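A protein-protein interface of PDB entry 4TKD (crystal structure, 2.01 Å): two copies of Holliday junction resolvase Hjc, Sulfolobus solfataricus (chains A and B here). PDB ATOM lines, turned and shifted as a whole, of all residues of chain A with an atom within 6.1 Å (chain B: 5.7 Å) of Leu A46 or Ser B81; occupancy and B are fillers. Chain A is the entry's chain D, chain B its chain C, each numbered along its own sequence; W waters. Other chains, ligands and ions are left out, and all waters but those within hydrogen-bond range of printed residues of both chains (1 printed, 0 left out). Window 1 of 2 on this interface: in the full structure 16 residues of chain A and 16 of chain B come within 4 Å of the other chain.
Among the printed residues, pairs that only touch across the chains: Gly A23 with Lys B80, Ala A25 with Phe B77, Ala A25 with Ser B81, Val A26 with Phe B77, Leu A46 with Lys B80, Leu A46 with Ser B81, Lys A47 with Lys B80, Lys A47 with Ser B81, Asn A48 with Ser B81, Gly A49 with Ile B51 and Gly A49 with Gly B82.
Of the printed residues of chain B, Gly A23 touches Lys B80 (3.5 Å).
Printed residues of chain B within 4 Å of Ala A25: Phe B77 and Ser B81.
Printed residues of chain B within 4 Å of Val A26: Phe B77 (3.7 Å).
Ala A45 touches none of the printed residues of chain B.
Leu A46 touches just these residues of chain B: Lys B80 and Ser B81.
Of the printed residues of chain A, Ile B51 touches Gly A49 (3.7 Å).
Ser B81 touches just these residues of chain A: Ala A25 (3.7 Å), Leu A46 (3.6 Å), Lys A47 (3.9 Å), Asn A48 (3.5 Å) and Gly A49 (2.8 Å).
Of the printed residues of chain A, Gly B82 touches Gly A49 (3.99 Å).
The nearest printed residue of chain B that does not touch Leu A46 is Ile B51 (4.1 Å).
The nearest residue of chain A that does not touch Ser B81 is Val A50 (4.5 Å).
Water W1 bridges O of Phe A24 and NZ of Lys B80.
Hydrophobic or aromatic side chains of chain A within 4 Å of the printed part of chain B: Ala A25 and Leu A46.
Printed residues of chain B that touch a printed residue of chain A: Ile B51, Phe B77, Lys B80, Ser B81 and Gly B82.
Among the printed residues, no Asp or Glu carboxylate lies within 4 Å of a Lys or Arg side-chain nitrogen of the other chain.
Positions printed for both chains: 44, 46 and 51.
O of Phe B77 lies within hydrogen-bond range of OG of Ser B81, at 2.9 Å.
The side-chain hydroxyl of Ser B81 sits at hydrogen-bond distance from the backbone carbonyl oxygen of Ala B78 (3.1 Å).
N of Gly B83 is in hydrogen-bond range of OG of Ser B81 (3.1 Å).
N of Leu A46 is in hydrogen-bond range of O of Ala A25, 2.7 Å away.
The backbone carbonyl oxygen of Lys B80 sits at hydrogen-bond distance from the backbone NH of Asn A48, at 3.0 Å.
O of Ser B81 lies within hydrogen-bond range of N of Gly A49 (2.8 Å).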
ATOM      1  N   GLY A  23     -13.247  32.435  15.252  1.00  0.00           N
ATOM      2  CA  GLY A  23     -12.439  32.256  14.049  1.00  0.00           C
ATOM      3  C   GLY A  23     -12.068  30.840  13.662  1.00  0.00           C
ATOM      4  O   GLY A  23     -11.118  30.648  12.905  1.00  0.00           O
ATOM      5  N   PHE A  24     -12.809  29.835  14.170  1.00  0.00           N
ATOM      6  CA  PHE A  24     -12.559  28.441  13.814  1.00  0.00           C
ATOM      7  C   PHE A  24     -13.410  28.045  12.617  1.00  0.00           C
ATOM      8  O   PHE A  24     -14.541  28.517  12.457  1.00  0.00           O
ATOM      9  CB  PHE A  24     -12.918  27.487  14.978  1.00  0.00           C
ATOM     10  CG  PHE A  24     -11.943  27.420  16.128  1.00  0.00           C
ATOM     11  CD1 PHE A  24     -11.883  28.443  17.074  1.00  0.00           C
ATOM     12  CD2 PHE A  24     -11.106  26.316  16.288  1.00  0.00           C
ATOM     13  CE1 PHE A  24     -10.993  28.370  18.157  1.00  0.00           C
ATOM     14  CE2 PHE A  24     -10.233  26.235  17.375  1.00  0.00           C
ATOM     15  CZ  PHE A  24     -10.196  27.261  18.312  1.00  0.00           C
ATOM     16  N   ALA A  25     -12.869  27.103  11.817  1.00  0.00           N
ATOM     17  CA  ALA A  25     -13.558  26.431  10.715  1.00  0.00           C
ATOM     18  C   ALA A  25     -14.092  25.193  11.416  1.00  0.00           C
ATOM     19  O   ALA A  25     -13.315  24.466  12.038  1.00  0.00           O
ATOM     20  CB  ALA A  25     -12.567  26.039   9.611  1.00  0.00           C
ATOM     21  N   VAL A  26     -15.426  24.997  11.402  1.00  0.00           N
ATOM     22  CA  VAL A  26     -16.073  23.908  12.158  1.00  0.00           C
ATOM     23  C   VAL A  26     -16.966  23.020  11.316  1.00  0.00           C
ATOM     24  O   VAL A  26     -17.763  23.506  10.515  1.00  0.00           O
ATOM     25  CB  VAL A  26     -16.871  24.454  13.401  1.00  0.00           C
ATOM     26  CG1 VAL A  26     -17.225  23.330  14.380  1.00  0.00           C
ATOM     27  CG2 VAL A  26     -16.102  25.542  14.135  1.00  0.00           C
ATOM     28  N   ILE A  44     -15.485  18.743  14.812  1.00  0.00           N
ATOM     29  CA  ILE A  44     -14.112  18.942  14.401  1.00  0.00           C
ATOM     30  C   ILE A  44     -13.974  20.449  14.160  1.00  0.00           C
ATOM     31  O   ILE A  44     -14.714  21.010  13.337  1.00  0.00           O
ATOM     32  CB  ILE A  44     -13.733  18.099  13.173  1.00  0.00           C
ATOM     33  CG1 ILE A  44     -13.842  16.579  13.499  1.00  0.00           C
ATOM     34  CG2 ILE A  44     -12.339  18.501  12.685  1.00  0.00           C
ATOM     35  CD1 ILE A  44     -14.119  15.667  12.337  1.00  0.00           C
ATOM     36  N   ALA A  45     -13.084  21.106  14.946  1.00  0.00           N
ATOM     37  CA  ALA A  45     -12.865  22.553  14.835  1.00  0.00           C
ATOM     38  C   ALA A  45     -11.412  22.807  14.511  1.00  0.00           C
ATOM     39  O   ALA A  45     -10.513  22.163  15.059  1.00  0.00           O
ATOM     40  CB  ALA A  45     -13.301  23.293  16.101  1.00  0.00           C
ATOM     41  N   LEU A  46     -11.191  23.667  13.519  1.00  0.00           N
ATOM     42  CA  LEU A  46      -9.853  23.920  13.017  1.00  0.00           C
ATOM     43  C   LEU A  46      -9.531  25.391  13.009  1.00  0.00           C
ATOM     44  O   LEU A  46     -10.346  26.184  12.544  1.00  0.00           O
ATOM     45  CB  LEU A  46      -9.679  23.325  11.602  1.00  0.00           C
ATOM     46  CG  LEU A  46     -10.313  21.960  11.274  1.00  0.00           C
ATOM     47  CD1 LEU A  46     -10.425  21.734   9.759  1.00  0.00           C
ATOM     48  CD2 LEU A  46      -9.547  20.819  11.942  1.00  0.00           C
ATOM     49  N   LYS A  47      -8.323  25.754  13.507  1.00  0.00           N
ATOM     50  CA  LYS A  47      -7.843  27.128  13.494  1.00  0.00           C
ATOM     51  C   LYS A  47      -6.331  27.195  13.375  1.00  0.00           C
ATOM     52  O   LYS A  47      -5.637  26.644  14.216  1.00  0.00           O
ATOM     53  CB  LYS A  47      -8.332  27.942  14.710  1.00  0.00           C
ATOM     54  CG  LYS A  47      -8.170  29.458  14.500  1.00  0.00           C
ATOM     55  CD  LYS A  47      -8.581  30.274  15.704  1.00  0.00           C
ATOM     56  CE  LYS A  47      -8.305  31.732  15.446  1.00  0.00           C
ATOM     57  NZ  LYS A  47      -8.834  32.608  16.535  1.00  0.00           N
ATOM     58  N   ASN A  48      -5.822  27.905  12.346  1.00  0.00           N
ATOM     59  CA  ASN A  48      -4.388  28.113  12.077  1.00  0.00           C
ATOM     60  C   ASN A  48      -3.546  26.827  12.189  1.00  0.00           C
ATOM     61  O   ASN A  48      -2.501  26.819  12.846  1.00  0.00           O
ATOM     62  CB  ASN A  48      -3.821  29.245  12.965  1.00  0.00           C
ATOM     63  CG  ASN A  48      -4.517  30.577  12.866  1.00  0.00           C
ATOM     64  OD1 ASN A  48      -4.660  31.287  13.865  1.00  0.00           O
ATOM     65  ND2 ASN A  48      -4.940  30.975  11.677  1.00  0.00           N
ATOM     66  N   GLY A  49      -4.033  25.756  11.574  1.00  0.00           N
ATOM     67  CA  GLY A  49      -3.385  24.444  11.584  1.00  0.00           C
ATOM     68  C   GLY A  49      -3.635  23.608  12.818  1.00  0.00           C
ATOM     69  O   GLY A  49      -3.135  22.489  12.888  1.00  0.00           O
ATOM     70  N   VAL A  50      -4.386  24.149  13.815  1.00  0.00           N
ATOM     71  CA  VAL A  50      -4.683  23.456  15.076  1.00  0.00           C
ATOM     72  C   VAL A  50      -6.042  22.754  15.037  1.00  0.00           C
ATOM     73  O   VAL A  50      -7.053  23.360  14.681  1.00  0.00           O
ATOM     74  CB  VAL A  50      -4.457  24.308  16.338  1.00  0.00           C
ATOM     75  CG1 VAL A  50      -4.717  23.490  17.606  1.00  0.00           C
ATOM     76  CG2 VAL A  50      -3.031  24.853  16.378  1.00  0.00           C
ATOM     77  N   ILE A  51      -6.032  21.464  15.392  1.00  0.00           N
ATOM     78  CA  ILE A  51      -7.183  20.580  15.403  1.00  0.00           C
ATOM     79  C   ILE A  51      -7.725  20.329  16.830  1.00  0.00           C
ATOM     80  O   ILE A  51      -6.998  19.890  17.717  1.00  0.00           O
ATOM     81  CB  ILE A  51      -6.858  19.269  14.631  1.00  0.00           C
ATOM     82  CG1 ILE A  51      -6.238  19.575  13.225  1.00  0.00           C
ATOM     83  CG2 ILE A  51      -8.066  18.354  14.525  1.00  0.00           C
ATOM     84  CD1 ILE A  51      -5.363  18.469  12.622  1.00  0.00           C
ATOM     85  N   ILE A  52      -9.014  20.641  17.021  1.00  0.00           N
ATOM     86  CA  ILE A  52      -9.768  20.373  18.229  1.00  0.00           C
ATOM     87  C   ILE A  52     -10.917  19.447  17.876  1.00  0.00           C
ATOM     88  O   ILE A  52     -11.594  19.649  16.860  1.00  0.00           O
ATOM     89  CB  ILE A  52     -10.151  21.610  19.065  1.00  0.00           C
ATOM     90  CG1 ILE A  52     -11.171  22.537  18.466  1.00  0.00           C
ATOM     91  CG2 ILE A  52      -8.906  22.319  19.624  1.00  0.00           C
ATOM     92  CD1 ILE A  52     -12.001  23.311  19.546  1.00  0.00           C
ATOM     93  N   ILE B  44     -12.448  16.295   4.175  1.00  0.00           N
ATOM     94  CA  ILE B  44     -11.507  16.884   5.099  1.00  0.00           C
ATOM     95  C   ILE B  44     -10.600  15.743   5.509  1.00  0.00           C
ATOM     96  O   ILE B  44     -11.074  14.741   6.039  1.00  0.00           O
ATOM     97  CB  ILE B  44     -12.185  17.578   6.310  1.00  0.00           C
ATOM     98  CG1 ILE B  44     -13.002  18.778   5.846  1.00  0.00           C
ATOM     99  CG2 ILE B  44     -11.145  18.016   7.352  1.00  0.00           C
ATOM    100  CD1 ILE B  44     -14.097  19.173   6.811  1.00  0.00           C
ATOM    101  N   LEU B  46      -7.028  14.757   7.567  1.00  0.00           N
ATOM    102  CA  LEU B  46      -6.103  15.243   8.580  1.00  0.00           C
ATOM    103  C   LEU B  46      -5.037  14.210   8.904  1.00  0.00           C
ATOM    104  O   LEU B  46      -5.348  13.026   9.057  1.00  0.00           O
ATOM    105  CB  LEU B  46      -6.861  15.598   9.876  1.00  0.00           C
ATOM    106  CG  LEU B  46      -8.193  16.335   9.761  1.00  0.00           C
ATOM    107  CD1 LEU B  46      -8.995  16.227  11.089  1.00  0.00           C
ATOM    108  CD2 LEU B  46      -7.987  17.802   9.280  1.00  0.00           C
ATOM    109  N   ILE B  51      -3.724  19.625   7.299  1.00  0.00           N
ATOM    110  CA  ILE B  51      -5.119  19.749   6.883  1.00  0.00           C
ATOM    111  C   ILE B  51      -5.203  19.871   5.372  1.00  0.00           C
ATOM    112  O   ILE B  51      -4.638  20.791   4.785  1.00  0.00           O
ATOM    113  CB  ILE B  51      -5.842  20.926   7.616  1.00  0.00           C
ATOM    114  CG1 ILE B  51      -5.681  20.828   9.166  1.00  0.00           C
ATOM    115  CG2 ILE B  51      -7.340  20.987   7.222  1.00  0.00           C
ATOM    116  CD1 ILE B  51      -5.812  22.140   9.930  1.00  0.00           C
ATOM    117  N   LEU B  53      -8.144  19.775   2.278  1.00  0.00           N
ATOM    118  CA  LEU B  53      -9.558  20.024   2.029  1.00  0.00           C
ATOM    119  C   LEU B  53      -9.825  19.839   0.546  1.00  0.00           C
ATOM    120  O   LEU B  53      -9.140  20.437  -0.271  1.00  0.00           O
ATOM    121  CB  LEU B  53      -9.936  21.469   2.479  1.00  0.00           C
ATOM    122  CG  LEU B  53      -9.533  21.864   3.906  1.00  0.00           C
ATOM    123  CD1 LEU B  53      -9.653  23.334   4.117  1.00  0.00           C
ATOM    124  CD2 LEU B  53     -10.349  21.112   4.929  1.00  0.00           C
ATOM    125  N   GLU B  76     -12.972  30.553   2.835  1.00  0.00           N
ATOM    126  CA  GLU B  76     -13.009  31.050   4.206  1.00  0.00           C
ATOM    127  C   GLU B  76     -12.724  29.917   5.228  1.00  0.00           C
ATOM    128  O   GLU B  76     -11.955  30.112   6.175  1.00  0.00           O
ATOM    129  CB  GLU B  76     -14.360  31.732   4.489  1.00  0.00           C
ATOM    130  CG  GLU B  76     -14.450  33.228   4.206  1.00  0.00           C
ATOM    131  CD  GLU B  76     -13.380  34.103   4.830  1.00  0.00           C
ATOM    132  OE1 GLU B  76     -12.361  34.308   4.142  1.00  0.00           O
ATOM    133  OE2 GLU B  76     -13.616  34.712   5.895  1.00  0.00           O
ATOM    134  N   PHE B  77     -13.316  28.739   5.011  1.00  0.00           N
ATOM    135  CA  PHE B  77     -13.088  27.546   5.849  1.00  0.00           C
ATOM    136  C   PHE B  77     -11.587  27.203   5.771  1.00  0.00           C
ATOM    137  O   PHE B  77     -10.964  27.030   6.813  1.00  0.00           O
ATOM    138  CB  PHE B  77     -13.944  26.366   5.326  1.00  0.00           C
ATOM    139  CG  PHE B  77     -14.018  25.128   6.188  1.00  0.00           C
ATOM    140  CD1 PHE B  77     -13.003  24.175   6.158  1.00  0.00           C
ATOM    141  CD2 PHE B  77     -15.116  24.907   7.021  1.00  0.00           C
ATOM    142  CE1 PHE B  77     -13.074  23.029   6.953  1.00  0.00           C
ATOM    143  CE2 PHE B  77     -15.176  23.768   7.832  1.00  0.00           C
ATOM    144  CZ  PHE B  77     -14.161  22.829   7.782  1.00  0.00           C
ATOM    145  N   ALA B  78     -11.005  27.167   4.535  1.00  0.00           N
ATOM    146  CA  ALA B  78      -9.582  26.907   4.279  1.00  0.00           C
ATOM    147  C   ALA B  78      -8.659  27.899   4.965  1.00  0.00           C
ATOM    148  O   ALA B  78      -7.647  27.488   5.534  1.00  0.00           O
ATOM    149  CB  ALA B  78      -9.302  26.897   2.786  1.00  0.00           C
ATOM    150  N   ARG B  79      -9.002  29.201   4.884  1.00  0.00           N
ATOM    151  CA  ARG B  79      -8.214  30.280   5.469  1.00  0.00           C
ATOM    152  C   ARG B  79      -8.204  30.188   7.014  1.00  0.00           C
ATOM    153  O   ARG B  79      -7.138  30.297   7.638  1.00  0.00           O
ATOM    154  CB  ARG B  79      -8.736  31.645   5.007  1.00  0.00           C
ATOM    155  CG  ARG B  79      -7.937  32.831   5.569  1.00  0.00           C
ATOM    156  CD  ARG B  79      -8.586  34.203   5.346  1.00  0.00           C
ATOM    157  NE  ARG B  79      -9.929  34.324   5.928  1.00  0.00           N
ATOM    158  CZ  ARG B  79     -10.190  34.519   7.216  1.00  0.00           C
ATOM    159  NH1 ARG B  79      -9.198  34.614   8.094  1.00  0.00           N
ATOM    160  NH2 ARG B  79     -11.441  34.604   7.639  1.00  0.00           N
ATOM    161  N   LYS B  80      -9.385  30.015   7.615  1.00  0.00           N
ATOM    162  CA  LYS B  80      -9.549  29.901   9.080  1.00  0.00           C
ATOM    163  C   LYS B  80      -8.878  28.668   9.633  1.00  0.00           C
ATOM    164  O   LYS B  80      -8.204  28.743  10.658  1.00  0.00           O
ATOM    165  CB  LYS B  80     -11.027  29.910   9.471  1.00  0.00           C
ATOM    166  CG  LYS B  80     -11.666  31.290   9.333  1.00  0.00           C
ATOM    167  CD  LYS B  80     -13.152  31.181   9.485  1.00  0.00           C
ATOM    168  CE  LYS B  80     -13.782  32.542   9.451  1.00  0.00           C
ATOM    169  NZ  LYS B  80     -15.250  32.432   9.302  1.00  0.00           N
ATOM    170  N   SER B  81      -9.039  27.530   8.949  1.00  0.00           N
ATOM    171  CA  SER B  81      -8.453  26.248   9.364  1.00  0.00           C
ATOM    172  C   SER B  81      -6.934  26.183   9.199  1.00  0.00           C
ATOM    173  O   SER B  81      -6.288  25.422   9.903  1.00  0.00           O
ATOM    174  CB  SER B  81      -9.093  25.103   8.581  1.00  0.00           C
ATOM    175  OG  SER B  81      -8.727  25.178   7.214  1.00  0.00           O
ATOM    176  N   GLY B  82      -6.401  26.918   8.229  1.00  0.00           N
ATOM    177  CA  GLY B  82      -4.989  26.876   7.871  1.00  0.00           C
ATOM    178  C   GLY B  82      -4.705  25.688   6.972  1.00  0.00           C
ATOM    179  O   GLY B  82      -3.546  25.290   6.824  1.00  0.00           O
ATOM    180  N   GLY B  83      -5.763  25.136   6.365  1.00  0.00           N
ATOM    181  CA  GLY B  83      -5.690  23.979   5.483  1.00  0.00           C
ATOM    182  C   GLY B  83      -5.411  24.301   4.031  1.00  0.00           C
ATOM    183  O   GLY B  83      -5.492  25.457   3.614  1.00  0.00           O
HETATM  184  O   HOH W   1     -15.433  31.014  11.876  1.00  0.00           O
